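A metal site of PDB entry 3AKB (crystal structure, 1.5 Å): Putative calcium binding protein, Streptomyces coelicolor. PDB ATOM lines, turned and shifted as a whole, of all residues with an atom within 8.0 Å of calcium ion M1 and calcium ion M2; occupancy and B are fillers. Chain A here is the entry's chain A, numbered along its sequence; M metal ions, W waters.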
ATOM      1  N   PHE A  10     -26.261 -17.028 -10.358  1.00  0.00           N
ATOM      2  CA  PHE A  10     -24.935 -16.756 -10.887  1.00  0.00           C
ATOM      3  C   PHE A  10     -24.126 -15.839  -9.974  1.00  0.00           C
ATOM      4  O   PHE A  10     -22.950 -16.094  -9.701  1.00  0.00           O
ATOM      5  CB  PHE A  10     -24.995 -16.163 -12.302  1.00  0.00           C
ATOM      6  CG  PHE A  10     -23.643 -15.979 -12.944  1.00  0.00           C
ATOM      7  CD1 PHE A  10     -22.992 -17.069 -13.508  1.00  0.00           C
ATOM      8  CD2 PHE A  10     -23.034 -14.743 -12.961  1.00  0.00           C
ATOM      9  CE1 PHE A  10     -21.717 -16.912 -14.081  1.00  0.00           C
ATOM     10  CE2 PHE A  10     -21.756 -14.585 -13.543  1.00  0.00           C
ATOM     11  CZ  PHE A  10     -21.116 -15.682 -14.102  1.00  0.00           C
ATOM     12  N   THR A  11     -24.751 -14.741  -9.531  1.00  0.00           N
ATOM     13  CA  THR A  11     -24.119 -13.777  -8.643  1.00  0.00           C
ATOM     14  C   THR A  11     -23.646 -14.416  -7.334  1.00  0.00           C
ATOM     15  O   THR A  11     -22.580 -14.056  -6.819  1.00  0.00           O
ATOM     16  CB  THR A  11     -25.088 -12.595  -8.346  1.00  0.00           C
ATOM     17  OG1 THR A  11     -25.451 -11.941  -9.575  1.00  0.00           O
ATOM     18  CG2 THR A  11     -24.461 -11.566  -7.417  1.00  0.00           C
ATOM     19  N   PHE A  13     -22.519 -17.365  -6.944  1.00  0.00           N
ATOM     20  CA  PHE A  13     -21.246 -18.070  -7.220  1.00  0.00           C
ATOM     21  C   PHE A  13     -20.125 -17.105  -7.610  1.00  0.00           C
ATOM     22  O   PHE A  13     -18.959 -17.305  -7.254  1.00  0.00           O
ATOM     23  CB  PHE A  13     -21.431 -19.093  -8.346  1.00  0.00           C
ATOM     24  CG  PHE A  13     -22.190 -20.348  -7.945  1.00  0.00           C
ATOM     25  CD1 PHE A  13     -21.827 -21.082  -6.818  1.00  0.00           C
ATOM     26  CD2 PHE A  13     -23.219 -20.823  -8.764  1.00  0.00           C
ATOM     27  CE1 PHE A  13     -22.542 -22.284  -6.488  1.00  0.00           C
ATOM     28  CE2 PHE A  13     -23.931 -22.014  -8.453  1.00  0.00           C
ATOM     29  CZ  PHE A  13     -23.582 -22.743  -7.310  1.00  0.00           C
ATOM     30  N   ASP A  14     -20.492 -16.047  -8.340  1.00  0.00           N
ATOM     31  CA  ASP A  14     -19.517 -15.049  -8.809  1.00  0.00           C
ATOM     32  C   ASP A  14     -19.262 -14.044  -7.707  1.00  0.00           C
ATOM     33  O   ASP A  14     -19.594 -12.859  -7.804  1.00  0.00           O
ATOM     34  CB  ASP A  14     -20.023 -14.377 -10.084  1.00  0.00           C
ATOM     35  CG  ASP A  14     -19.027 -13.396 -10.657  1.00  0.00           C
ATOM     36  OD1 ASP A  14     -17.806 -13.559 -10.370  1.00  0.00           O
ATOM     37  OD2 ASP A  14     -19.447 -12.460 -11.398  1.00  0.00           O
ATOM     38  N   GLN A  15     -18.577 -14.528  -6.664  1.00  0.00           N
ATOM     39  CA  GLN A  15     -18.349 -13.776  -5.445  1.00  0.00           C
ATOM     40  C   GLN A  15     -17.611 -12.464  -5.656  1.00  0.00           C
ATOM     41  O   GLN A  15     -17.913 -11.482  -4.970  1.00  0.00           O
ATOM     42  CB  GLN A  15     -17.646 -14.665  -4.421  1.00  0.00           C
ATOM     43  CG  GLN A  15     -18.584 -15.707  -3.795  1.00  0.00           C
ATOM     44  CD  GLN A  15     -19.475 -15.112  -2.715  1.00  0.00           C
ATOM     45  OE1 GLN A  15     -18.981 -14.433  -1.814  1.00  0.00           O
ATOM     46  NE2 GLN A  15     -20.770 -15.383  -2.767  1.00  0.00           N
ATOM     47  N   ASP A  16     -16.666 -12.415  -6.611  1.00  0.00           N
ATOM     48  CA  ASP A  16     -15.929 -11.173  -6.868  1.00  0.00           C
ATOM     49  C   ASP A  16     -16.565 -10.273  -7.947  1.00  0.00           C
ATOM     50  O   ASP A  16     -16.070  -9.177  -8.244  1.00  0.00           O
ATOM     51  CB  ASP A  16     -14.434 -11.470  -7.130  1.00  0.00           C
ATOM     52  CG  ASP A  16     -14.181 -12.161  -8.450  1.00  0.00           C
ATOM     53  OD1 ASP A  16     -15.072 -12.225  -9.330  1.00  0.00           O
ATOM     54  OD2 ASP A  16     -13.021 -12.615  -8.609  1.00  0.00           O
ATOM     55  N   GLY A  17     -17.679 -10.731  -8.490  1.00  0.00           N
ATOM     56  CA  GLY A  17     -18.512  -9.919  -9.387  1.00  0.00           C
ATOM     57  C   GLY A  17     -17.989  -9.673 -10.780  1.00  0.00           C
ATOM     58  O   GLY A  17     -18.524  -8.822 -11.501  1.00  0.00           O
ATOM     59  N   ASN A  18     -16.955 -10.417 -11.192  1.00  0.00           N
ATOM     60  CA  ASN A  18     -16.274 -10.074 -12.436  1.00  0.00           C
ATOM     61  C   ASN A  18     -16.825 -10.795 -13.698  1.00  0.00           C
ATOM     62  O   ASN A  18     -16.238 -10.721 -14.792  1.00  0.00           O
ATOM     63  CB  ASN A  18     -14.777 -10.289 -12.256  1.00  0.00           C
ATOM     64  CG  ASN A  18     -14.405 -11.757 -12.251  1.00  0.00           C
ATOM     65  OD1 ASN A  18     -15.248 -12.651 -12.241  1.00  0.00           O
ATOM     66  ND2 ASN A  18     -13.112 -12.007 -12.312  1.00  0.00           N
ATOM     67  N   GLY A  19     -17.965 -11.461 -13.542  1.00  0.00           N
ATOM     68  CA  GLY A  19     -18.701 -12.018 -14.690  1.00  0.00           C
ATOM     69  C   GLY A  19     -18.382 -13.437 -15.097  1.00  0.00           C
ATOM     70  O   GLY A  19     -18.989 -13.989 -16.023  1.00  0.00           O
ATOM     71  N   HIS A  20     -17.427 -14.056 -14.391  1.00  0.00           N
ATOM     72  CA  HIS A  20     -17.195 -15.463 -14.604  1.00  0.00           C
ATOM     73  C   HIS A  20     -16.834 -16.087 -13.270  1.00  0.00           C
ATOM     74  O   HIS A  20     -16.304 -15.414 -12.397  1.00  0.00           O
ATOM     75  CB  HIS A  20     -16.097 -15.708 -15.663  1.00  0.00           C
ATOM     76  CG  HIS A  20     -14.727 -15.216 -15.280  1.00  0.00           C
ATOM     77  ND1 HIS A  20     -14.202 -14.031 -15.740  1.00  0.00           N
ATOM     78  CD2 HIS A  20     -13.763 -15.809 -14.532  1.00  0.00           C
ATOM     79  CE1 HIS A  20     -12.981 -13.878 -15.258  1.00  0.00           C
ATOM     80  NE2 HIS A  20     -12.676 -14.957 -14.539  1.00  0.00           N
ATOM     81  N   ILE A  21     -17.130 -17.370 -13.127  1.00  0.00           N
ATOM     82  CA  ILE A  21     -16.870 -18.102 -11.882  1.00  0.00           C
ATOM     83  C   ILE A  21     -15.528 -18.835 -12.027  1.00  0.00           C
ATOM     84  O   ILE A  21     -15.335 -19.576 -13.002  1.00  0.00           O
ATOM     85  CB  ILE A  21     -17.993 -19.097 -11.588  1.00  0.00           C
ATOM     86  CG1 ILE A  21     -19.338 -18.360 -11.534  1.00  0.00           C
ATOM     87  CG2 ILE A  21     -17.721 -19.806 -10.254  1.00  0.00           C
ATOM     88  CD1 ILE A  21     -20.559 -19.225 -11.775  1.00  0.00           C
ATOM     89  N   ASP A  22     -14.626 -18.578 -11.068  1.00  0.00           N
ATOM     90  CA  ASP A  22     -13.285 -19.177 -10.945  1.00  0.00           C
ATOM     91  C   ASP A  22     -13.166 -19.931  -9.627  1.00  0.00           C
ATOM     92  O   ASP A  22     -13.938 -19.683  -8.687  1.00  0.00           O
ATOM     93  CB  ASP A  22     -12.190 -18.093 -10.778  1.00  0.00           C
ATOM     94  CG  ASP A  22     -11.868 -17.346 -12.025  1.00  0.00           C
ATOM     95  OD1 ASP A  22     -11.793 -17.913 -13.145  1.00  0.00           O
ATOM     96  OD2 ASP A  22     -11.654 -16.122 -11.845  1.00  0.00           O
ATOM     97  N   ARG A  23     -12.140 -20.768  -9.516  1.00  0.00           N
ATOM     98  CA  ARG A  23     -11.843 -21.369  -8.221  1.00  0.00           C
ATOM     99  C   ARG A  23     -11.651 -20.262  -7.191  1.00  0.00           C
ATOM    100  O   ARG A  23     -12.024 -20.428  -6.050  1.00  0.00           O
ATOM    101  CB  ARG A  23     -10.609 -22.268  -8.277  1.00  0.00           C
ATOM    102  CG  ARG A  23     -10.434 -23.091  -7.008  1.00  0.00           C
ATOM    103  CD  ARG A  23      -9.161 -23.887  -7.051  1.00  0.00           C
ATOM    104  NE  ARG A  23      -8.024 -23.035  -6.774  1.00  0.00           N
ATOM    105  CZ  ARG A  23      -6.808 -23.494  -6.489  1.00  0.00           C
ATOM    106  NH1 ARG A  23      -6.572 -24.808  -6.482  1.00  0.00           N
ATOM    107  NH2 ARG A  23      -5.846 -22.621  -6.251  1.00  0.00           N
ATOM    108  N   SER A  24     -11.074 -19.144  -7.603  1.00  0.00           N
ATOM    109  CA  SER A  24     -10.767 -18.049  -6.675  1.00  0.00           C
ATOM    110  C   SER A  24     -12.029 -17.413  -6.077  1.00  0.00           C
ATOM    111  O   SER A  24     -11.996 -16.862  -4.974  1.00  0.00           O
ATOM    112  CB  SER A  24      -9.896 -16.979  -7.297  1.00  0.00           C
ATOM    113  OG  SER A  24     -10.533 -16.414  -8.405  1.00  0.00           O
ATOM    114  N   ASP A  25     -13.159 -17.496  -6.774  1.00  0.00           N
ATOM    115  CA  ASP A  25     -14.416 -17.004  -6.184  1.00  0.00           C
ATOM    116  C   ASP A  25     -14.742 -17.801  -4.936  1.00  0.00           C
ATOM    117  O   ASP A  25     -15.157 -17.235  -3.906  1.00  0.00           O
ATOM    118  CB  ASP A  25     -15.574 -17.146  -7.174  1.00  0.00           C
ATOM    119  CG  ASP A  25     -15.615 -16.065  -8.257  1.00  0.00           C
ATOM    120  OD1 ASP A  25     -15.641 -14.842  -7.937  1.00  0.00           O
ATOM    121  OD2 ASP A  25     -15.652 -16.442  -9.460  1.00  0.00           O
ATOM    122  N   PHE A  26     -14.543 -19.111  -5.036  1.00  0.00           N
ATOM    123  CA  PHE A  26     -14.818 -20.059  -3.932  1.00  0.00           C
ATOM    124  C   PHE A  26     -13.801 -19.938  -2.801  1.00  0.00           C
ATOM    125  O   PHE A  26     -14.189 -19.914  -1.627  1.00  0.00           O
ATOM    126  CB  PHE A  26     -14.871 -21.487  -4.480  1.00  0.00           C
ATOM    127  CG  PHE A  26     -16.125 -21.787  -5.249  1.00  0.00           C
ATOM    128  CD1 PHE A  26     -17.213 -22.406  -4.620  1.00  0.00           C
ATOM    129  CD2 PHE A  26     -16.219 -21.490  -6.624  1.00  0.00           C
ATOM    130  CE1 PHE A  26     -18.370 -22.689  -5.316  1.00  0.00           C
ATOM    131  CE2 PHE A  26     -17.397 -21.773  -7.307  1.00  0.00           C
ATOM    132  CZ  PHE A  26     -18.471 -22.364  -6.645  1.00  0.00           C
ATOM    133  N   ASP A  69     -11.706 -24.412 -19.735  1.00  0.00           N
ATOM    134  CA  ASP A  69     -10.736 -23.373 -19.423  1.00  0.00           C
ATOM    135  C   ASP A  69     -10.772 -22.972 -17.949  1.00  0.00           C
ATOM    136  O   ASP A  69     -10.061 -22.044 -17.556  1.00  0.00           O
ATOM    137  CB  ASP A  69     -10.902 -22.152 -20.344  1.00  0.00           C
ATOM    138  CG  ASP A  69     -12.168 -21.346 -20.071  1.00  0.00           C
ATOM    139  OD1 ASP A  69     -13.096 -21.831 -19.367  1.00  0.00           O
ATOM    140  OD2 ASP A  69     -12.229 -20.187 -20.578  1.00  0.00           O
ATOM    141  N   GLN A  70     -11.592 -23.658 -17.142  1.00  0.00           N
ATOM    142  CA  GLN A  70     -11.631 -23.420 -15.683  1.00  0.00           C
ATOM    143  C   GLN A  70     -12.073 -22.003 -15.303  1.00  0.00           C
ATOM    144  O   GLN A  70     -11.653 -21.426 -14.287  1.00  0.00           O
ATOM    145  CB  GLN A  70     -10.287 -23.864 -15.051  1.00  0.00           C
ATOM    146  CG  GLN A  70     -10.073 -25.381 -15.210  1.00  0.00           C
ATOM    147  CD  GLN A  70      -8.668 -25.857 -14.845  1.00  0.00           C
ATOM    148  OE1 GLN A  70      -7.774 -25.058 -14.562  1.00  0.00           O
ATOM    149  NE2 GLN A  70      -8.483 -27.174 -14.864  1.00  0.00           N
ATOM    150  N   ARG A  71     -12.907 -21.429 -16.170  1.00  0.00           N
ATOM    151  CA  ARG A  71     -13.713 -20.233 -15.925  1.00  0.00           C
ATOM    152  C   ARG A  71     -15.124 -20.641 -16.371  1.00  0.00           C
ATOM    153  O   ARG A  71     -15.297 -21.280 -17.433  1.00  0.00           O
ATOM    154  CB  ARG A  71     -13.255 -19.041 -16.767  1.00  0.00           C
ATOM    155  CG  ARG A  71     -11.879 -18.478 -16.416  1.00  0.00           C
ATOM    156  CD  ARG A  71     -11.555 -17.255 -17.263  1.00  0.00           C
ATOM    157  NE  ARG A  71     -11.277 -17.680 -18.620  1.00  0.00           N
ATOM    158  CZ  ARG A  71     -10.047 -17.888 -19.090  1.00  0.00           C
ATOM    159  NH1 ARG A  71      -9.011 -17.679 -18.286  1.00  0.00           N
ATOM    160  NH2 ARG A  71      -9.876 -18.280 -20.338  1.00  0.00           N
ATOM    161  N   ILE A  72     -16.126 -20.317 -15.568  1.00  0.00           N
ATOM    162  CA  ILE A  72     -17.512 -20.545 -15.986  1.00  0.00           C
ATOM    163  C   ILE A  72     -18.115 -19.195 -16.315  1.00  0.00           C
ATOM    164  O   ILE A  72     -18.318 -18.367 -15.434  1.00  0.00           O
ATOM    165  CB  ILE A  72     -18.353 -21.187 -14.856  1.00  0.00           C
ATOM    166  CG1 ILE A  72     -17.718 -22.521 -14.418  1.00  0.00           C
ATOM    167  CG2 ILE A  72     -19.804 -21.383 -15.323  1.00  0.00           C
ATOM    168  CD1 ILE A  72     -18.261 -23.058 -13.079  1.00  0.00           C
HETATM  169 CA    CA M   1     -15.640 -14.227 -10.468  1.00  0.00          CA
HETATM  170 CA    CA M   2     -10.939 -15.197 -13.636  1.00  0.00          CA
HETATM  171  O   HOH W   1     -13.297 -14.475 -10.516  1.00  0.00           O
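The side-chain carboxylate (OD1) of Asp 14 lies close to the backbone NH (N) of Gly 17 (3.4 Å). OD1 of Asp 25 sits close to N of Gln 15 (3.2 Å). N of Asp 22 lies close to OD2 of Asp 25, at 2.9 Å. N of Gly 19 is in hydrogen-bond range of OD2 of Asp 14.
Five residues have an atom within 4 Å of calcium ion M1: Asp 14, Asp 16, Asn 18, His 20 and Asp 25.
Calcium ion M1 is bound by the side-chain carboxylate (OD1) of Asp 14 (2.3 Å), water W1 (2.4 Å), the backbone carbonyl oxygen (O) of His 20 (2.4 Å), the side-chain carboxylate (OD1) of Asp 16 (2.4 Å), the side-chain amide oxygen (OD1) of Asn 18 (2.4 Å), the side-chain carboxylate (OD2) of Asp 25 (2.4 Å) and the side-chain carboxylate (OD1) of Asp 25 (2.6 Å).
Calcium ion M2 is bound by NE2 of His 20 (2.0 Å), OD2 of Asp 22 (2.1 Å) and OD1 of Asp 22 (2.9 Å). Calcium ion M2 has three donor atoms within binding distance.
Water W1 bridges the side-chain carboxylate of Asp 16 and the side-chain amide nitrogen of Asn 18.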
